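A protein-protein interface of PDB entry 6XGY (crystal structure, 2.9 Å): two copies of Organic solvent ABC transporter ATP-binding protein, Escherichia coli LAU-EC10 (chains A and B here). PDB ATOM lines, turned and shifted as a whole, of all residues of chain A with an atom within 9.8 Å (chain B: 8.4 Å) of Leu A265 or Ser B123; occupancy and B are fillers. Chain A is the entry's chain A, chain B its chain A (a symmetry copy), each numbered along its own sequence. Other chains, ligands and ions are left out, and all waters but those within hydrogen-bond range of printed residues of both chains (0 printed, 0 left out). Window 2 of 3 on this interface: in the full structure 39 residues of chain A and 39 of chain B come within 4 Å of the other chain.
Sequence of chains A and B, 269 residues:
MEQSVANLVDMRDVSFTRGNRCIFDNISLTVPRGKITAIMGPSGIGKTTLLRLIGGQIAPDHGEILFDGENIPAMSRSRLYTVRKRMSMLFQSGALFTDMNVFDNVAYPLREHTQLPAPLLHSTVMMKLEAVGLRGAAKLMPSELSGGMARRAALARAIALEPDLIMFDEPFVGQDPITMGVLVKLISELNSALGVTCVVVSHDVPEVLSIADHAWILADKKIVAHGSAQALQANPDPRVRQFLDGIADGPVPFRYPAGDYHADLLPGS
The backbone carbonyl oxygen (O) of Asp A260 sits at hydrogen-bond distance from the guanidinium group (NH1) of Arg B135 (3.5 Å). OD2 of Asp A264 lies within salt-bridge range of NH1 of Arg B135, at 2.5 Å. O of Leu A265 lies within hydrogen-bond range of OG of Ser B123 (2.9 Å). NH2 of Arg B135 lies within hydrogen-bond range of O of Gly A259, 3.2 Å away.
The side-chain carboxylate (OD2) of Asp A260 sits at hydrogen-bond distance from the backbone NH (N) of Ala A263, 3.1 Å away. O of Pro B119 is in hydrogen-bond range of OG of Ser B123 (3.2 Å). The guanidinium group of Arg B135 is in salt-bridge range of the side-chain carboxylate of Glu B130, 2.8 Å away.
Tyr A261 touches Met B126 (OH to O, 3.9 Å). Met B127 touches Tyr A261. OH of Tyr A261 touches CB of Glu B130, at 3.4 Å. Tyr A261 touches Arg B135 (CD1 to NE, 3.4 Å). CG of Met B126 touches O of Asp A264 (3.5 Å). Met B127 touches Leu A265.
Leu A265 touches two residues of chain B. Ser B123 touches just one residue of chain A: Leu A265. Printed residues of chain A within 4 Å of Glu B130: Tyr A261. Of the printed residues of chain A, Met B126 touches Tyr A261 and Asp A264. Of the printed residues of chain B, Asp A264 touches Met B126 and Arg B135. Ala B118 touches none of the printed residues of chain A. The nearest residue of chain B that does not touch Leu A265 is Met B126 (4.2 Å).
Of the 18 printed residues of chain B, 5 touch a printed residue of chain A. Of the 10 printed residues of chain A, 5 touch a printed residue of chain B. Printed residues of chain A that touch a printed residue of chain B: Gly A259, Asp A260, Tyr A261, Asp A264 and Leu A265.
No position is printed for both chains.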
ATOM      1  N   GLY A 259     -32.426   2.999  -9.252  1.00  0.00           N
ATOM      2  CA  GLY A 259     -33.343   2.103  -8.579  1.00  0.00           C
ATOM      3  C   GLY A 259     -33.532   2.468  -7.122  1.00  0.00           C
ATOM      4  O   GLY A 259     -33.366   3.630  -6.741  1.00  0.00           O
ATOM      5  N   ASP A 260     -33.864   1.482  -6.292  1.00  0.00           N
ATOM      6  CA  ASP A 260     -34.242   1.750  -4.911  1.00  0.00           C
ATOM      7  C   ASP A 260     -33.004   2.027  -4.066  1.00  0.00           C
ATOM      8  O   ASP A 260     -32.123   1.169  -3.938  1.00  0.00           O
ATOM      9  CB  ASP A 260     -35.031   0.579  -4.334  1.00  0.00           C
ATOM     10  CG  ASP A 260     -35.642   0.908  -2.992  1.00  0.00           C
ATOM     11  OD1 ASP A 260     -36.472   1.838  -2.932  1.00  0.00           O
ATOM     12  OD2 ASP A 260     -35.289   0.247  -1.995  1.00  0.00           O
ATOM     13  N   TYR A 261     -32.955   3.221  -3.472  1.00  0.00           N
ATOM     14  CA  TYR A 261     -31.811   3.608  -2.652  1.00  0.00           C
ATOM     15  C   TYR A 261     -31.775   2.829  -1.342  1.00  0.00           C
ATOM     16  O   TYR A 261     -30.703   2.391  -0.907  1.00  0.00           O
ATOM     17  CB  TYR A 261     -31.863   5.114  -2.385  1.00  0.00           C
ATOM     18  CG  TYR A 261     -30.583   5.734  -1.859  1.00  0.00           C
ATOM     19  CD1 TYR A 261     -29.409   4.997  -1.757  1.00  0.00           C
ATOM     20  CD2 TYR A 261     -30.555   7.065  -1.461  1.00  0.00           C
ATOM     21  CE1 TYR A 261     -28.246   5.568  -1.275  1.00  0.00           C
ATOM     22  CE2 TYR A 261     -29.398   7.643  -0.978  1.00  0.00           C
ATOM     23  CZ  TYR A 261     -28.247   6.892  -0.888  1.00  0.00           C
ATOM     24  OH  TYR A 261     -27.095   7.466  -0.408  1.00  0.00           O
ATOM     25  N   HIS A 262     -32.933   2.643  -0.702  1.00  0.00           N
ATOM     26  CA  HIS A 262     -32.960   2.013   0.616  1.00  0.00           C
ATOM     27  C   HIS A 262     -32.364   0.612   0.576  1.00  0.00           C
ATOM     28  O   HIS A 262     -31.669   0.199   1.512  1.00  0.00           O
ATOM     29  CB  HIS A 262     -34.393   1.974   1.149  1.00  0.00           C
ATOM     30  CG  HIS A 262     -34.513   1.384   2.521  1.00  0.00           C
ATOM     31  ND1 HIS A 262     -34.529   0.024   2.749  1.00  0.00           N
ATOM     32  CD2 HIS A 262     -34.629   1.969   3.736  1.00  0.00           C
ATOM     33  CE1 HIS A 262     -34.645  -0.202   4.045  1.00  0.00           C
ATOM     34  NE2 HIS A 262     -34.709   0.962   4.666  1.00  0.00           N
ATOM     35  N   ALA A 263     -32.612  -0.131  -0.505  1.00  0.00           N
ATOM     36  CA  ALA A 263     -32.069  -1.481  -0.610  1.00  0.00           C
ATOM     37  C   ALA A 263     -30.554  -1.460  -0.786  1.00  0.00           C
ATOM     38  O   ALA A 263     -29.851  -2.326  -0.252  1.00  0.00           O
ATOM     39  CB  ALA A 263     -32.737  -2.229  -1.763  1.00  0.00           C
ATOM     40  N   ASP A 264     -30.030  -0.480  -1.529  1.00  0.00           N
ATOM     41  CA  ASP A 264     -28.586  -0.405  -1.740  1.00  0.00           C
ATOM     42  C   ASP A 264     -27.841  -0.089  -0.452  1.00  0.00           C
ATOM     43  O   ASP A 264     -26.674  -0.471  -0.305  1.00  0.00           O
ATOM     44  CB  ASP A 264     -28.255   0.640  -2.804  1.00  0.00           C
ATOM     45  CG  ASP A 264     -28.525   0.145  -4.212  1.00  0.00           C
ATOM     46  OD1 ASP A 264     -28.557  -1.089  -4.414  1.00  0.00           O
ATOM     47  OD2 ASP A 264     -28.696   0.990  -5.117  1.00  0.00           O
ATOM     48  N   LEU A 265     -28.487   0.608   0.482  1.00  0.00           N
ATOM     49  CA  LEU A 265     -27.841   0.931   1.748  1.00  0.00           C
ATOM     50  C   LEU A 265     -27.928  -0.227   2.734  1.00  0.00           C
ATOM     51  O   LEU A 265     -26.953  -0.527   3.431  1.00  0.00           O
ATOM     52  CB  LEU A 265     -28.472   2.184   2.352  1.00  0.00           C
ATOM     53  CG  LEU A 265     -28.164   3.512   1.666  1.00  0.00           C
ATOM     54  CD1 LEU A 265     -29.211   4.552   2.022  1.00  0.00           C
ATOM     55  CD2 LEU A 265     -26.783   3.990   2.073  1.00  0.00           C
ATOM     56  N   LEU A 266     -29.083  -0.887   2.800  1.00  0.00           N
ATOM     57  CA  LEU A 266     -29.377  -1.881   3.830  1.00  0.00           C
ATOM     58  C   LEU A 266     -29.850  -3.163   3.158  1.00  0.00           C
ATOM     59  O   LEU A 266     -31.047  -3.329   2.883  1.00  0.00           O
ATOM     60  CB  LEU A 266     -30.423  -1.347   4.806  1.00  0.00           C
ATOM     61  CG  LEU A 266     -30.241   0.130   5.178  1.00  0.00           C
ATOM     62  CD1 LEU A 266     -31.521   0.721   5.739  1.00  0.00           C
ATOM     63  CD2 LEU A 266     -29.093   0.304   6.158  1.00  0.00           C
ATOM     64  N   PRO A 267     -28.936  -4.098   2.875  1.00  0.00           N
ATOM     65  CA  PRO A 267     -29.333  -5.332   2.187  1.00  0.00           C
ATOM     66  C   PRO A 267     -29.703  -6.453   3.145  1.00  0.00           C
ATOM     67  O   PRO A 267     -30.861  -6.573   3.560  1.00  0.00           O
ATOM     68  CB  PRO A 267     -28.086  -5.691   1.365  1.00  0.00           C
ATOM     69  CG  PRO A 267     -26.989  -4.703   1.797  1.00  0.00           C
ATOM     70  CD  PRO A 267     -27.478  -4.022   3.035  1.00  0.00           C
ATOM     71  N   GLY A 268     -28.727  -7.283   3.494  1.00  0.00           N
ATOM     72  CA  GLY A 268     -28.963  -8.408   4.381  1.00  0.00           C
ATOM     73  C   GLY A 268     -27.993  -8.471   5.544  1.00  0.00           C
ATOM     74  O   GLY A 268     -28.403  -8.547   6.703  1.00  0.00           O
ATOM     75  N   PHE B 103     -17.904   0.988  -8.213  1.00  0.00           N
ATOM     76  CA  PHE B 103     -18.031   0.753  -6.780  1.00  0.00           C
ATOM     77  C   PHE B 103     -16.705   0.294  -6.186  1.00  0.00           C
ATOM     78  O   PHE B 103     -16.249   0.833  -5.170  1.00  0.00           O
ATOM     79  CB  PHE B 103     -19.132  -0.276  -6.516  1.00  0.00           C
ATOM     80  CG  PHE B 103     -19.350  -0.570  -5.059  1.00  0.00           C
ATOM     81  CD1 PHE B 103     -18.674  -1.607  -4.439  1.00  0.00           C
ATOM     82  CD2 PHE B 103     -20.230   0.194  -4.311  1.00  0.00           C
ATOM     83  CE1 PHE B 103     -18.870  -1.877  -3.103  1.00  0.00           C
ATOM     84  CE2 PHE B 103     -20.431  -0.072  -2.972  1.00  0.00           C
ATOM     85  CZ  PHE B 103     -19.749  -1.108  -2.367  1.00  0.00           C
ATOM     86  N   LEU B 110     -10.894   2.567   1.315  1.00  0.00           N
ATOM     87  CA  LEU B 110     -11.353   2.162   2.639  1.00  0.00           C
ATOM     88  C   LEU B 110     -11.132   0.673   2.884  1.00  0.00           C
ATOM     89  O   LEU B 110     -10.936   0.261   4.033  1.00  0.00           O
ATOM     90  CB  LEU B 110     -12.831   2.510   2.808  1.00  0.00           C
ATOM     91  CG  LEU B 110     -13.211   3.980   2.634  1.00  0.00           C
ATOM     92  CD1 LEU B 110     -14.437   4.103   1.742  1.00  0.00           C
ATOM     93  CD2 LEU B 110     -13.463   4.638   3.987  1.00  0.00           C
ATOM     94  N   LEU B 116     -12.594   0.052   9.238  1.00  0.00           N
ATOM     95  CA  LEU B 116     -14.040   0.094   9.365  1.00  0.00           C
ATOM     96  C   LEU B 116     -14.625  -1.267   8.995  1.00  0.00           C
ATOM     97  O   LEU B 116     -14.133  -1.921   8.077  1.00  0.00           O
ATOM     98  CB  LEU B 116     -14.608   1.172   8.449  1.00  0.00           C
ATOM     99  CG  LEU B 116     -16.114   1.418   8.329  1.00  0.00           C
ATOM    100  CD1 LEU B 116     -16.617   2.090   9.589  1.00  0.00           C
ATOM    101  CD2 LEU B 116     -16.379   2.285   7.107  1.00  0.00           C
ATOM    102  N   PRO B 117     -15.658  -1.727   9.707  1.00  0.00           N
ATOM    103  CA  PRO B 117     -16.310  -2.992   9.336  1.00  0.00           C
ATOM    104  C   PRO B 117     -16.899  -2.961   7.933  1.00  0.00           C
ATOM    105  O   PRO B 117     -17.129  -1.911   7.327  1.00  0.00           O
ATOM    106  CB  PRO B 117     -17.417  -3.151  10.388  1.00  0.00           C
ATOM    107  CG  PRO B 117     -17.600  -1.782  10.970  1.00  0.00           C
ATOM    108  CD  PRO B 117     -16.219  -1.201  10.963  1.00  0.00           C
ATOM    109  N   ALA B 118     -17.188  -4.175   7.437  1.00  0.00           N
ATOM    110  CA  ALA B 118     -17.570  -4.343   6.035  1.00  0.00           C
ATOM    111  C   ALA B 118     -18.948  -3.773   5.721  1.00  0.00           C
ATOM    112  O   ALA B 118     -19.055  -2.982   4.768  1.00  0.00           O
ATOM    113  CB  ALA B 118     -17.462  -5.819   5.645  1.00  0.00           C
ATOM    114  N   PRO B 119     -20.028  -4.121   6.436  1.00  0.00           N
ATOM    115  CA  PRO B 119     -21.344  -3.584   6.044  1.00  0.00           C
ATOM    116  C   PRO B 119     -21.425  -2.070   6.117  1.00  0.00           C
ATOM    117  O   PRO B 119     -22.185  -1.470   5.350  1.00  0.00           O
ATOM    118  CB  PRO B 119     -22.308  -4.246   7.040  1.00  0.00           C
ATOM    119  CG  PRO B 119     -21.593  -5.450   7.524  1.00  0.00           C
ATOM    120  CD  PRO B 119     -20.150  -5.044   7.577  1.00  0.00           C
ATOM    121  N   LEU B 120     -20.668  -1.435   7.016  1.00  0.00           N
ATOM    122  CA  LEU B 120     -20.665   0.024   7.068  1.00  0.00           C
ATOM    123  C   LEU B 120     -19.850   0.610   5.925  1.00  0.00           C
ATOM    124  O   LEU B 120     -20.199   1.665   5.381  1.00  0.00           O
ATOM    125  CB  LEU B 120     -20.119   0.504   8.413  1.00  0.00           C
ATOM    126  CG  LEU B 120     -20.929   0.078   9.639  1.00  0.00           C
ATOM    127  CD1 LEU B 120     -20.360   0.716  10.885  1.00  0.00           C
ATOM    128  CD2 LEU B 120     -22.399   0.439   9.459  1.00  0.00           C
ATOM    129  N   LEU B 121     -18.750  -0.051   5.561  1.00  0.00           N
ATOM    130  CA  LEU B 121     -17.982   0.369   4.394  1.00  0.00           C
ATOM    131  C   LEU B 121     -18.845   0.335   3.139  1.00  0.00           C
ATOM    132  O   LEU B 121     -18.790   1.252   2.312  1.00  0.00           O
ATOM    133  CB  LEU B 121     -16.749  -0.528   4.241  1.00  0.00           C
ATOM    134  CG  LEU B 121     -15.594  -0.093   3.335  1.00  0.00           C
ATOM    135  CD1 LEU B 121     -14.309  -0.749   3.806  1.00  0.00           C
ATOM    136  CD2 LEU B 121     -15.860  -0.445   1.876  1.00  0.00           C
ATOM    137  N   HIS B 122     -19.657  -0.715   2.991  1.00  0.00           N
ATOM    138  CA  HIS B 122     -20.518  -0.839   1.819  1.00  0.00           C
ATOM    139  C   HIS B 122     -21.519   0.307   1.749  1.00  0.00           C
ATOM    140  O   HIS B 122     -21.712   0.914   0.690  1.00  0.00           O
ATOM    141  CB  HIS B 122     -21.239  -2.187   1.848  1.00  0.00           C
ATOM    142  CG  HIS B 122     -21.833  -2.584   0.533  1.00  0.00           C
ATOM    143  ND1 HIS B 122     -21.123  -3.277  -0.424  1.00  0.00           N
ATOM    144  CD2 HIS B 122     -23.068  -2.387   0.015  1.00  0.00           C
ATOM    145  CE1 HIS B 122     -21.895  -3.491  -1.474  1.00  0.00           C
ATOM    146  NE2 HIS B 122     -23.080  -2.960  -1.234  1.00  0.00           N
ATOM    147  N   SER B 123     -22.169   0.617   2.875  1.00  0.00           N
ATOM    148  CA  SER B 123     -23.100   1.740   2.904  1.00  0.00           C
ATOM    149  C   SER B 123     -22.389   3.063   2.651  1.00  0.00           C
ATOM    150  O   SER B 123     -22.979   3.983   2.073  1.00  0.00           O
ATOM    151  CB  SER B 123     -23.830   1.781   4.247  1.00  0.00           C
ATOM    152  OG  SER B 123     -24.467   0.546   4.525  1.00  0.00           O
ATOM    153  N   THR B 124     -21.128   3.177   3.074  1.00  0.00           N
ATOM    154  CA  THR B 124     -20.399   4.432   2.918  1.00  0.00           C
ATOM    155  C   THR B 124     -20.124   4.736   1.451  1.00  0.00           C
ATOM    156  O   THR B 124     -20.221   5.892   1.021  1.00  0.00           O
ATOM    157  CB  THR B 124     -19.088   4.378   3.698  1.00  0.00           C
ATOM    158  OG1 THR B 124     -19.341   3.914   5.029  1.00  0.00           O
ATOM    159  CG2 THR B 124     -18.452   5.759   3.761  1.00  0.00           C
ATOM    160  N   VAL B 125     -19.768   3.715   0.672  1.00  0.00           N
ATOM    161  CA  VAL B 125     -19.514   3.930  -0.748  1.00  0.00           C
ATOM    162  C   VAL B 125     -20.812   4.258  -1.476  1.00  0.00           C
ATOM    163  O   VAL B 125     -20.839   5.122  -2.361  1.00  0.00           O
ATOM    164  CB  VAL B 125     -18.808   2.703  -1.352  1.00  0.00           C
ATOM    165  CG1 VAL B 125     -18.426   2.965  -2.801  1.00  0.00           C
ATOM    166  CG2 VAL B 125     -17.579   2.350  -0.533  1.00  0.00           C
ATOM    167  N   MET B 126     -21.907   3.586  -1.108  1.00  0.00           N
ATOM    168  CA  MET B 126     -23.201   3.888  -1.713  1.00  0.00           C
ATOM    169  C   MET B 126     -23.585   5.347  -1.494  1.00  0.00           C
ATOM    170  O   MET B 126     -24.074   6.013  -2.414  1.00  0.00           O
ATOM    171  CB  MET B 126     -24.278   2.962  -1.149  1.00  0.00           C
ATOM    172  CG  MET B 126     -24.220   1.539  -1.675  1.00  0.00           C
ATOM    173  SD  MET B 126     -24.391   1.475  -3.469  1.00  0.00           S
ATOM    174  CE  MET B 126     -24.519  -0.290  -3.744  1.00  0.00           C
ATOM    175  N   MET B 127     -23.371   5.859  -0.280  1.00  0.00           N
ATOM    176  CA  MET B 127     -23.686   7.256  -0.003  1.00  0.00           C
ATOM    177  C   MET B 127     -22.812   8.187  -0.834  1.00  0.00           C
ATOM    178  O   MET B 127     -23.306   9.144  -1.443  1.00  0.00           O
ATOM    179  CB  MET B 127     -23.524   7.547   1.491  1.00  0.00           C
ATOM    180  CG  MET B 127     -24.568   6.884   2.375  1.00  0.00           C
ATOM    181  SD  MET B 127     -24.520   7.450   4.091  1.00  0.00           S
ATOM    182  CE  MET B 127     -22.947   6.792   4.633  1.00  0.00           C
ATOM    183  N   LYS B 128     -21.506   7.916  -0.882  1.00  0.00           N
ATOM    184  CA  LYS B 128     -20.604   8.795  -1.618  1.00  0.00           C
ATOM    185  C   LYS B 128     -20.834   8.711  -3.124  1.00  0.00           C
ATOM    186  O   LYS B 128     -20.584   9.689  -3.841  1.00  0.00           O
ATOM    187  CB  LYS B 128     -19.154   8.476  -1.257  1.00  0.00           C
ATOM    188  CG  LYS B 128     -18.717   9.148   0.036  1.00  0.00           C
ATOM    189  CD  LYS B 128     -17.453   8.548   0.619  1.00  0.00           C
ATOM    190  CE  LYS B 128     -17.076   9.258   1.914  1.00  0.00           C
ATOM    191  NZ  LYS B 128     -16.039   8.517   2.688  1.00  0.00           N
ATOM    192  N   LEU B 129     -21.314   7.572  -3.626  1.00  0.00           N
ATOM    193  CA  LEU B 129     -21.712   7.517  -5.029  1.00  0.00           C
ATOM    194  C   LEU B 129     -22.962   8.347  -5.283  1.00  0.00           C
ATOM    195  O   LEU B 129     -23.108   8.936  -6.361  1.00  0.00           O
ATOM    196  CB  LEU B 129     -21.934   6.070  -5.466  1.00  0.00           C
ATOM    197  CG  LEU B 129     -20.678   5.207  -5.591  1.00  0.00           C
ATOM    198  CD1 LEU B 129     -21.026   3.821  -6.113  1.00  0.00           C
ATOM    199  CD2 LEU B 129     -19.659   5.882  -6.492  1.00  0.00           C
ATOM    200  N   GLU B 130     -23.872   8.406  -4.307  1.00  0.00           N
ATOM    201  CA  GLU B 130     -25.038   9.271  -4.432  1.00  0.00           C
ATOM    202  C   GLU B 130     -24.644  10.742  -4.372  1.00  0.00           C
ATOM    203  O   GLU B 130     -25.330  11.591  -4.954  1.00  0.00           O
ATOM    204  CB  GLU B 130     -26.052   8.936  -3.335  1.00  0.00           C
ATOM    205  CG  GLU B 130     -27.390   9.658  -3.440  1.00  0.00           C
ATOM    206  CD  GLU B 130     -28.292   9.083  -4.514  1.00  0.00           C
ATOM    207  OE1 GLU B 130     -29.355   9.681  -4.783  1.00  0.00           O
ATOM    208  OE2 GLU B 130     -27.943   8.029  -5.085  1.00  0.00           O
ATOM    209  N   ARG B 135     -24.683   6.504  -8.383  1.00  0.00           N
ATOM    210  CA  ARG B 135     -25.036   5.259  -7.710  1.00  0.00           C
ATOM    211  C   ARG B 135     -25.546   4.218  -8.698  1.00  0.00           C
ATOM    212  O   ARG B 135     -25.336   3.016  -8.497  1.00  0.00           O
ATOM    213  CB  ARG B 135     -26.073   5.525  -6.617  1.00  0.00           C
ATOM    214  CG  ARG B 135     -26.465   4.286  -5.822  1.00  0.00           C
ATOM    215  CD  ARG B 135     -27.338   4.631  -4.622  1.00  0.00           C
ATOM    216  NE  ARG B 135     -28.599   5.262  -5.007  1.00  0.00           N
ATOM    217  CZ  ARG B 135     -29.707   4.595  -5.317  1.00  0.00           C
ATOM    218  NH1 ARG B 135     -29.716   3.269  -5.294  1.00  0.00           N
ATOM    219  NH2 ARG B 135     -30.808   5.257  -5.652  1.00  0.00           N
